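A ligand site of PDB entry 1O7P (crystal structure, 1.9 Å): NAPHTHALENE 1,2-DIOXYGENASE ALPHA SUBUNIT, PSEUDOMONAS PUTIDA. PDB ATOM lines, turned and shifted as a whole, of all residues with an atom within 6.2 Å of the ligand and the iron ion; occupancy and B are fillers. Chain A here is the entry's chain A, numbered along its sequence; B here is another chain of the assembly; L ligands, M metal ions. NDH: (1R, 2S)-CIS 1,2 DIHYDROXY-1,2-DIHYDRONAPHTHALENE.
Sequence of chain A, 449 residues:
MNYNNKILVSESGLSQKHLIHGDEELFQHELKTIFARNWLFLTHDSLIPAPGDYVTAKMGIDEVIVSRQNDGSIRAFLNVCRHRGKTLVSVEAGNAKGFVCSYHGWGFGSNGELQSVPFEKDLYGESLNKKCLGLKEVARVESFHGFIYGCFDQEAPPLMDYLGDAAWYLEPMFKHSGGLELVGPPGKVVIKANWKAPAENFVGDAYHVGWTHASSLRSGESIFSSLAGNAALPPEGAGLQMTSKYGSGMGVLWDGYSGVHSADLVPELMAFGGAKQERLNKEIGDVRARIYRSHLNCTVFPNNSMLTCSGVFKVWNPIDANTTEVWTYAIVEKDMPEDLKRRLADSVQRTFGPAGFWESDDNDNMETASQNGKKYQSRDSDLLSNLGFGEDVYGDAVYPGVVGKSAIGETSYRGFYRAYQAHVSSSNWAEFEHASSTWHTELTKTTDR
Residues that only touch the iron ion: Asn 201 (3.8 Å).
Of the 23 residues printed, 4 come within 4 Å of the iron ion.
The iron ion is bound by NE2 of His 208 (2.0 Å), NE2 of His 213 (2.0 Å), OD2 of Asp 362 (2.1 Å) and OD1 of Asp 362 (2.2 Å).
Slightly farther from the iron ion lies OH2 of the ligand (2.8 Å).
Slightly farther from the iron ion lies an oxygen (OH1) of the ligand (2.8 Å).
An oxygen (OH1) of the ligand sits close to a ring nitrogen (NE2) of His 208.
An oxygen (OH2) of the ligand lies close to a ring nitrogen (NE2) of His 213.
ND2 of Asn 201 lies within hydrogen-bond range of OH1 of the ligand (2.7 Å).
Phe 202 touches the ligand (CE1 to OH1, 3.7 Å).
O of Asp 205 touches C4 of the ligand, at 3.6 Å.
CG2 of Val 209 touches C4A of the ligand, 3.7 Å away.
Leu 253 touches the ligand (CD2 to C6, 3.996 Å).
His 295 touches the ligand (CE1 to C6, 3.5 Å).
ND2 of Asn 297 touches C4 of the ligand, 3.8 Å away.
Phe 352 touches the ligand.
Hydrophobic or aromatic side chains within 4 Å of the ligand: Phe 202, His 208, Val 209, His 213, Leu 253, His 295 and Phe 352.
11 residues have an atom within 4 Å of the ligand: Asn 201, Phe 202, Asp 205, His 208, Val 209, His 213, Leu 253, His 295, Asn 297, Phe 352 and Asp 362.
OD1 of Asn 201 sits at hydrogen-bond distance from OH of Tyr 103 of chain B (3.2 Å).
OD1 of Asp 205 lies close to OD1 of Asn 201 (3.3 Å).
O of Phe 202 sits at hydrogen-bond distance from ND2 of Asn 297, at 3.0 Å.
A ring nitrogen (ND1) of His 208 is in hydrogen-bond range of the backbone carbonyl oxygen (O) of Asp 205.
The backbone carbonyl oxygen of His 295 lies within hydrogen-bond range of the backbone NH of Leu 253 (3.0 Å).
A ring nitrogen (ND1) of His 213 is in hydrogen-bond range of the side-chain carboxylate (OD1) of Asp 361, at 2.9 Å.
A ring nitrogen (ND1) of His 213 lies close to the backbone carbonyl oxygen (O) of Trp 358 (3.3 Å).
The side-chain amide oxygen (OD1) of Asn 201 lies close to a ring nitrogen (ND1) of His 208 (3.5 Å).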
ATOM      1  N   ASN A 201      18.478  14.570 -10.663  1.00  0.00           N
ATOM      2  CA  ASN A 201      18.059  14.133 -11.963  1.00  0.00           C
ATOM      3  C   ASN A 201      17.953  12.622 -11.979  1.00  0.00           C
ATOM      4  O   ASN A 201      16.943  12.061 -12.460  1.00  0.00           O
ATOM      5  CB  ASN A 201      19.051  14.639 -13.029  1.00  0.00           C
ATOM      6  CG  ASN A 201      18.710  14.139 -14.433  1.00  0.00           C
ATOM      7  OD1 ASN A 201      17.772  14.657 -15.069  1.00  0.00           O
ATOM      8  ND2 ASN A 201      19.435  13.159 -14.906  1.00  0.00           N
ATOM      9  N   PHE A 202      18.978  11.953 -11.446  1.00  0.00           N
ATOM     10  CA  PHE A 202      18.979  10.492 -11.330  1.00  0.00           C
ATOM     11  C   PHE A 202      17.998   9.980 -10.257  1.00  0.00           C
ATOM     12  O   PHE A 202      17.471   8.868 -10.391  1.00  0.00           O
ATOM     13  CB  PHE A 202      20.368   9.916 -11.051  1.00  0.00           C
ATOM     14  CG  PHE A 202      21.180   9.672 -12.296  1.00  0.00           C
ATOM     15  CD1 PHE A 202      21.566  10.726 -13.086  1.00  0.00           C
ATOM     16  CD2 PHE A 202      21.503   8.405 -12.706  1.00  0.00           C
ATOM     17  CE1 PHE A 202      22.260  10.525 -14.250  1.00  0.00           C
ATOM     18  CE2 PHE A 202      22.254   8.198 -13.865  1.00  0.00           C
ATOM     19  CZ  PHE A 202      22.622   9.288 -14.640  1.00  0.00           C
ATOM     20  N   VAL A 203      17.774  10.728  -9.186  1.00  0.00           N
ATOM     21  CA  VAL A 203      16.879  10.206  -8.130  1.00  0.00           C
ATOM     22  C   VAL A 203      15.431  10.166  -8.527  1.00  0.00           C
ATOM     23  O   VAL A 203      14.704   9.299  -8.043  1.00  0.00           O
ATOM     24  CB  VAL A 203      16.962  10.990  -6.835  1.00  0.00           C
ATOM     25  CG1 VAL A 203      15.941  12.131  -6.822  1.00  0.00           C
ATOM     26  CG2 VAL A 203      16.745  10.078  -5.644  1.00  0.00           C
ATOM     27  N   ASP A 205      13.934  11.817 -11.926  1.00  0.00           N
ATOM     28  CA  ASP A 205      13.555  12.556 -13.098  1.00  0.00           C
ATOM     29  C   ASP A 205      13.263  11.710 -14.323  1.00  0.00           C
ATOM     30  O   ASP A 205      14.083  11.606 -15.215  1.00  0.00           O
ATOM     31  CB  ASP A 205      14.641  13.568 -13.442  1.00  0.00           C
ATOM     32  CG  ASP A 205      14.083  14.634 -14.348  1.00  0.00           C
ATOM     33  OD1 ASP A 205      14.692  15.725 -14.423  1.00  0.00           O
ATOM     34  OD2 ASP A 205      13.025  14.380 -14.970  1.00  0.00           O
ATOM     35  N   ALA A 206      12.078  11.090 -14.378  1.00  0.00           N
ATOM     36  CA  ALA A 206      11.701  10.413 -15.632  1.00  0.00           C
ATOM     37  C   ALA A 206      11.051  11.376 -16.621  1.00  0.00           C
ATOM     38  O   ALA A 206      10.980  11.085 -17.822  1.00  0.00           O
ATOM     39  CB  ALA A 206      10.794   9.218 -15.363  1.00  0.00           C
ATOM     40  N   HIS A 208      12.039  14.145 -17.813  1.00  0.00           N
ATOM     41  CA  HIS A 208      12.960  14.756 -18.810  1.00  0.00           C
ATOM     42  C   HIS A 208      13.379  13.826 -19.938  1.00  0.00           C
ATOM     43  O   HIS A 208      13.827  14.276 -21.003  1.00  0.00           O
ATOM     44  CB  HIS A 208      14.236  15.319 -18.111  1.00  0.00           C
ATOM     45  CG  HIS A 208      15.366  14.335 -17.983  1.00  0.00           C
ATOM     46  ND1 HIS A 208      15.342  13.262 -17.121  1.00  0.00           N
ATOM     47  CD2 HIS A 208      16.570  14.286 -18.600  1.00  0.00           C
ATOM     48  CE1 HIS A 208      16.471  12.590 -17.219  1.00  0.00           C
ATOM     49  NE2 HIS A 208      17.244  13.191 -18.115  1.00  0.00           N
ATOM     50  N   VAL A 209      13.224  12.523 -19.716  1.00  0.00           N
ATOM     51  CA  VAL A 209      13.807  11.513 -20.631  1.00  0.00           C
ATOM     52  C   VAL A 209      13.339  11.654 -22.064  1.00  0.00           C
ATOM     53  O   VAL A 209      14.165  11.706 -22.985  1.00  0.00           O
ATOM     54  CB  VAL A 209      13.629  10.101 -20.094  1.00  0.00           C
ATOM     55  CG1 VAL A 209      14.112   9.062 -21.122  1.00  0.00           C
ATOM     56  CG2 VAL A 209      14.426   9.957 -18.757  1.00  0.00           C
ATOM     57  N   THR A 212      14.573  15.717 -23.148  1.00  0.00           N
ATOM     58  CA  THR A 212      16.029  15.886 -23.114  1.00  0.00           C
ATOM     59  C   THR A 212      16.730  14.867 -24.008  1.00  0.00           C
ATOM     60  O   THR A 212      17.632  15.220 -24.773  1.00  0.00           O
ATOM     61  CB  THR A 212      16.560  15.707 -21.697  1.00  0.00           C
ATOM     62  OG1 THR A 212      16.229  16.863 -20.909  1.00  0.00           O
ATOM     63  CG2 THR A 212      18.092  15.681 -21.710  1.00  0.00           C
ATOM     64  N   HIS A 213      16.314  13.609 -23.928  1.00  0.00           N
ATOM     65  CA  HIS A 213      17.014  12.537 -24.643  1.00  0.00           C
ATOM     66  C   HIS A 213      16.331  12.135 -25.955  1.00  0.00           C
ATOM     67  O   HIS A 213      16.600  11.057 -26.489  1.00  0.00           O
ATOM     68  CB  HIS A 213      17.213  11.332 -23.741  1.00  0.00           C
ATOM     69  CG  HIS A 213      18.079  11.601 -22.543  1.00  0.00           C
ATOM     70  ND1 HIS A 213      19.440  11.810 -22.644  1.00  0.00           N
ATOM     71  CD2 HIS A 213      17.779  11.715 -21.223  1.00  0.00           C
ATOM     72  CE1 HIS A 213      19.940  12.036 -21.430  1.00  0.00           C
ATOM     73  NE2 HIS A 213      18.952  11.949 -20.556  1.00  0.00           N
ATOM     74  N   PHE A 224      13.399   2.078 -24.670  1.00  0.00           N
ATOM     75  CA  PHE A 224      12.568   3.218 -24.333  1.00  0.00           C
ATOM     76  C   PHE A 224      12.365   4.186 -25.486  1.00  0.00           C
ATOM     77  O   PHE A 224      11.811   5.268 -25.295  1.00  0.00           O
ATOM     78  CB  PHE A 224      13.167   3.918 -23.140  1.00  0.00           C
ATOM     79  CG  PHE A 224      13.206   3.068 -21.917  1.00  0.00           C
ATOM     80  CD1 PHE A 224      12.072   2.348 -21.548  1.00  0.00           C
ATOM     81  CD2 PHE A 224      14.358   2.947 -21.156  1.00  0.00           C
ATOM     82  CE1 PHE A 224      12.078   1.561 -20.442  1.00  0.00           C
ATOM     83  CE2 PHE A 224      14.365   2.145 -20.033  1.00  0.00           C
ATOM     84  CZ  PHE A 224      13.225   1.452 -19.676  1.00  0.00           C
ATOM     85  N   LEU A 253      10.872   1.527 -13.641  1.00  0.00           N
ATOM     86  CA  LEU A 253      10.268   1.456 -14.956  1.00  0.00           C
ATOM     87  C   LEU A 253      10.134  -0.034 -15.232  1.00  0.00           C
ATOM     88  O   LEU A 253      11.094  -0.683 -15.640  1.00  0.00           O
ATOM     89  CB  LEU A 253      11.127   2.113 -16.019  1.00  0.00           C
ATOM     90  CG  LEU A 253      10.675   3.484 -16.550  1.00  0.00           C
ATOM     91  CD1 LEU A 253      10.237   4.388 -15.398  1.00  0.00           C
ATOM     92  CD2 LEU A 253      11.790   4.144 -17.365  1.00  0.00           C
ATOM     93  N   VAL A 260      19.101   1.598 -21.428  1.00  0.00           N
ATOM     94  CA  VAL A 260      19.467   2.561 -22.480  1.00  0.00           C
ATOM     95  C   VAL A 260      20.256   1.918 -23.606  1.00  0.00           C
ATOM     96  O   VAL A 260      20.559   2.574 -24.589  1.00  0.00           O
ATOM     97  CB  VAL A 260      20.310   3.711 -21.902  1.00  0.00           C
ATOM     98  CG1 VAL A 260      19.559   4.370 -20.811  1.00  0.00           C
ATOM     99  CG2 VAL A 260      21.662   3.210 -21.413  1.00  0.00           C
ATOM    100  N   HIS A 295      14.051  -1.382 -14.613  1.00  0.00           N
ATOM    101  CA  HIS A 295      15.073  -0.323 -14.624  1.00  0.00           C
ATOM    102  C   HIS A 295      14.848   0.637 -13.479  1.00  0.00           C
ATOM    103  O   HIS A 295      13.805   1.274 -13.402  1.00  0.00           O
ATOM    104  CB  HIS A 295      14.922   0.383 -15.959  1.00  0.00           C
ATOM    105  CG  HIS A 295      16.078   1.217 -16.359  1.00  0.00           C
ATOM    106  ND1 HIS A 295      16.114   2.577 -16.148  1.00  0.00           N
ATOM    107  CD2 HIS A 295      17.210   0.914 -17.056  1.00  0.00           C
ATOM    108  CE1 HIS A 295      17.222   3.081 -16.682  1.00  0.00           C
ATOM    109  NE2 HIS A 295      17.918   2.079 -17.217  1.00  0.00           N
ATOM    110  N   ASN A 297      16.208   3.961 -11.577  1.00  0.00           N
ATOM    111  CA  ASN A 297      17.081   5.136 -11.602  1.00  0.00           C
ATOM    112  C   ASN A 297      17.091   5.641 -10.171  1.00  0.00           C
ATOM    113  O   ASN A 297      16.114   6.171  -9.672  1.00  0.00           O
ATOM    114  CB  ASN A 297      16.617   6.193 -12.624  1.00  0.00           C
ATOM    115  CG  ASN A 297      15.239   6.672 -12.383  1.00  0.00           C
ATOM    116  OD1 ASN A 297      14.271   5.977 -12.661  1.00  0.00           O
ATOM    117  ND2 ASN A 297      15.124   7.923 -11.913  1.00  0.00           N
ATOM    118  N   LEU A 307      21.826   3.433 -12.584  1.00  0.00           N
ATOM    119  CA  LEU A 307      20.744   2.966 -13.416  1.00  0.00           C
ATOM    120  C   LEU A 307      20.881   1.451 -13.462  1.00  0.00           C
ATOM    121  O   LEU A 307      21.723   0.949 -14.203  1.00  0.00           O
ATOM    122  CB  LEU A 307      20.812   3.498 -14.824  1.00  0.00           C
ATOM    123  CG  LEU A 307      20.837   5.006 -15.048  1.00  0.00           C
ATOM    124  CD1 LEU A 307      20.946   5.318 -16.544  1.00  0.00           C
ATOM    125  CD2 LEU A 307      19.602   5.655 -14.427  1.00  0.00           C
ATOM    126  N   SER A 310      20.611  -1.018 -17.096  1.00  0.00           N
ATOM    127  CA  SER A 310      21.494  -0.297 -17.954  1.00  0.00           C
ATOM    128  C   SER A 310      22.930  -0.499 -17.442  1.00  0.00           C
ATOM    129  O   SER A 310      23.878  -0.577 -18.240  1.00  0.00           O
ATOM    130  CB  SER A 310      21.180   1.210 -17.935  1.00  0.00           C
ATOM    131  OG  SER A 310      20.113   1.524 -18.808  1.00  0.00           O
ATOM    132  N   PHE A 352      26.683   6.668 -21.361  1.00  0.00           N
ATOM    133  CA  PHE A 352      26.784   7.535 -20.190  1.00  0.00           C
ATOM    134  C   PHE A 352      28.188   7.924 -19.741  1.00  0.00           C
ATOM    135  O   PHE A 352      28.321   8.650 -18.725  1.00  0.00           O
ATOM    136  CB  PHE A 352      25.967   6.929 -19.036  1.00  0.00           C
ATOM    137  CG  PHE A 352      24.536   7.255 -19.130  1.00  0.00           C
ATOM    138  CD1 PHE A 352      24.064   8.406 -18.528  1.00  0.00           C
ATOM    139  CD2 PHE A 352      23.673   6.509 -19.872  1.00  0.00           C
ATOM    140  CE1 PHE A 352      22.747   8.770 -18.644  1.00  0.00           C
ATOM    141  CE2 PHE A 352      22.355   6.849 -19.991  1.00  0.00           C
ATOM    142  CZ  PHE A 352      21.883   7.967 -19.388  1.00  0.00           C
ATOM    143  N   TRP A 358      24.107   9.903 -24.505  1.00  0.00           N
ATOM    144  CA  TRP A 358      22.970  10.267 -23.649  1.00  0.00           C
ATOM    145  C   TRP A 358      23.382  11.332 -22.643  1.00  0.00           C
ATOM    146  O   TRP A 358      22.669  12.321 -22.477  1.00  0.00           O
ATOM    147  CB  TRP A 358      22.407   9.079 -22.843  1.00  0.00           C
ATOM    148  CG  TRP A 358      21.755   8.036 -23.629  1.00  0.00           C
ATOM    149  CD1 TRP A 358      22.300   7.244 -24.613  1.00  0.00           C
ATOM    150  CD2 TRP A 358      20.386   7.598 -23.484  1.00  0.00           C
ATOM    151  NE1 TRP A 358      21.361   6.365 -25.089  1.00  0.00           N
ATOM    152  CE2 TRP A 358      20.173   6.567 -24.415  1.00  0.00           C
ATOM    153  CE3 TRP A 358      19.339   7.967 -22.636  1.00  0.00           C
ATOM    154  CZ2 TRP A 358      18.944   5.908 -24.533  1.00  0.00           C
ATOM    155  CZ3 TRP A 358      18.110   7.308 -22.754  1.00  0.00           C
ATOM    156  CH2 TRP A 358      17.922   6.310 -23.698  1.00  0.00           C
ATOM    157  N   ASP A 361      23.392  14.957 -23.657  1.00  0.00           N
ATOM    158  CA  ASP A 361      22.091  15.621 -23.712  1.00  0.00           C
ATOM    159  C   ASP A 361      21.804  16.420 -22.422  1.00  0.00           C
ATOM    160  O   ASP A 361      21.103  17.405 -22.468  1.00  0.00           O
ATOM    161  CB  ASP A 361      20.963  14.590 -23.860  1.00  0.00           C
ATOM    162  CG  ASP A 361      21.033  13.773 -25.180  1.00  0.00           C
ATOM    163  OD1 ASP A 361      20.464  12.656 -25.204  1.00  0.00           O
ATOM    164  OD2 ASP A 361      21.629  14.158 -26.215  1.00  0.00           O
ATOM    165  N   ASP A 362      22.296  15.915 -21.285  1.00  0.00           N
ATOM    166  CA  ASP A 362      21.975  16.489 -19.977  1.00  0.00           C
ATOM    167  C   ASP A 362      22.902  17.617 -19.539  1.00  0.00           C
ATOM    168  O   ASP A 362      22.579  18.351 -18.597  1.00  0.00           O
ATOM    169  CB  ASP A 362      22.075  15.427 -18.882  1.00  0.00           C
ATOM    170  CG  ASP A 362      20.959  14.425 -18.921  1.00  0.00           C
ATOM    171  OD1 ASP A 362      21.291  13.225 -19.041  1.00  0.00           O
ATOM    172  OD2 ASP A 362      19.765  14.719 -18.810  1.00  0.00           O
ATOM    173  N   ASN A 365      21.506  21.202 -19.486  1.00  0.00           N
ATOM    174  CA  ASN A 365      20.478  21.290 -18.474  1.00  0.00           C
ATOM    175  C   ASN A 365      21.102  21.463 -17.095  1.00  0.00           C
ATOM    176  O   ASN A 365      20.693  22.327 -16.318  1.00  0.00           O
ATOM    177  CB  ASN A 365      19.628  20.014 -18.438  1.00  0.00           C
ATOM    178  CG  ASN A 365      18.848  19.775 -19.735  1.00  0.00           C
ATOM    179  OD1 ASN A 365      18.582  20.688 -20.506  1.00  0.00           O
ATOM    180  ND2 ASN A 365      18.528  18.525 -19.982  1.00  0.00           N
ATOM    181  N   MET A 366      22.054  20.626 -16.775  1.00  0.00           N
ATOM    182  CA  MET A 366      22.614  20.675 -15.438  1.00  0.00           C
ATOM    183  C   MET A 366      23.472  21.894 -15.210  1.00  0.00           C
ATOM    184  O   MET A 366      23.406  22.540 -14.172  1.00  0.00           O
ATOM    185  CB  MET A 366      23.510  19.474 -15.151  1.00  0.00           C
ATOM    186  CG  MET A 366      23.016  18.179 -15.756  1.00  0.00           C
ATOM    187  SD  MET A 366      21.867  17.331 -14.672  1.00  0.00           S
ATOM    188  CE  MET A 366      22.543  15.668 -14.673  1.00  0.00           C
ATOM    189  N   TYR B 103      14.803  20.934 -21.053  1.00  0.00           N
ATOM    190  CA  TYR B 103      14.934  19.966 -19.989  1.00  0.00           C
ATOM    191  C   TYR B 103      13.686  19.050 -19.921  1.00  0.00           C
ATOM    192  O   TYR B 103      13.780  17.847 -20.200  1.00  0.00           O
ATOM    193  CB  TYR B 103      15.217  20.681 -18.652  1.00  0.00           C
ATOM    194  CG  TYR B 103      15.885  19.875 -17.550  1.00  0.00           C
ATOM    195  CD1 TYR B 103      16.341  20.527 -16.413  1.00  0.00           C
ATOM    196  CD2 TYR B 103      16.017  18.487 -17.586  1.00  0.00           C
ATOM    197  CE1 TYR B 103      16.934  19.839 -15.385  1.00  0.00           C
ATOM    198  CE2 TYR B 103      16.596  17.774 -16.556  1.00  0.00           C
ATOM    199  CZ  TYR B 103      17.062  18.450 -15.446  1.00  0.00           C
ATOM    200  OH  TYR B 103      17.675  17.774 -14.425  1.00  0.00           O
HETATM  201  OH2 NDH L   1      18.784   9.942 -18.464  1.00  0.00           O
HETATM  202  C1  NDH L   1      18.447   8.915 -17.468  1.00  0.00           C
HETATM  203  C2  NDH L   1      18.839   9.594 -16.116  1.00  0.00           C
HETATM  204  OH1 NDH L   1      19.329  10.912 -16.473  1.00  0.00           O
HETATM  205  C3  NDH L   1      17.679   9.634 -15.121  1.00  0.00           C
HETATM  206  C4  NDH L   1      16.533   8.903 -15.315  1.00  0.00           C
HETATM  207  C4A NDH L   1      16.429   7.847 -16.431  1.00  0.00           C
HETATM  208  C8A NDH L   1      17.372   7.818 -17.490  1.00  0.00           C
HETATM  209  C8  NDH L   1      17.293   6.888 -18.513  1.00  0.00           C
HETATM  210  C5  NDH L   1      15.417   6.873 -16.411  1.00  0.00           C
HETATM  211  C6  NDH L   1      15.365   5.929 -17.430  1.00  0.00           C
HETATM  212  C7  NDH L   1      16.281   5.933 -18.478  1.00  0.00           C
HETATM  213 FE    FE M   1      19.148  12.675 -18.654  1.00  0.00          FE
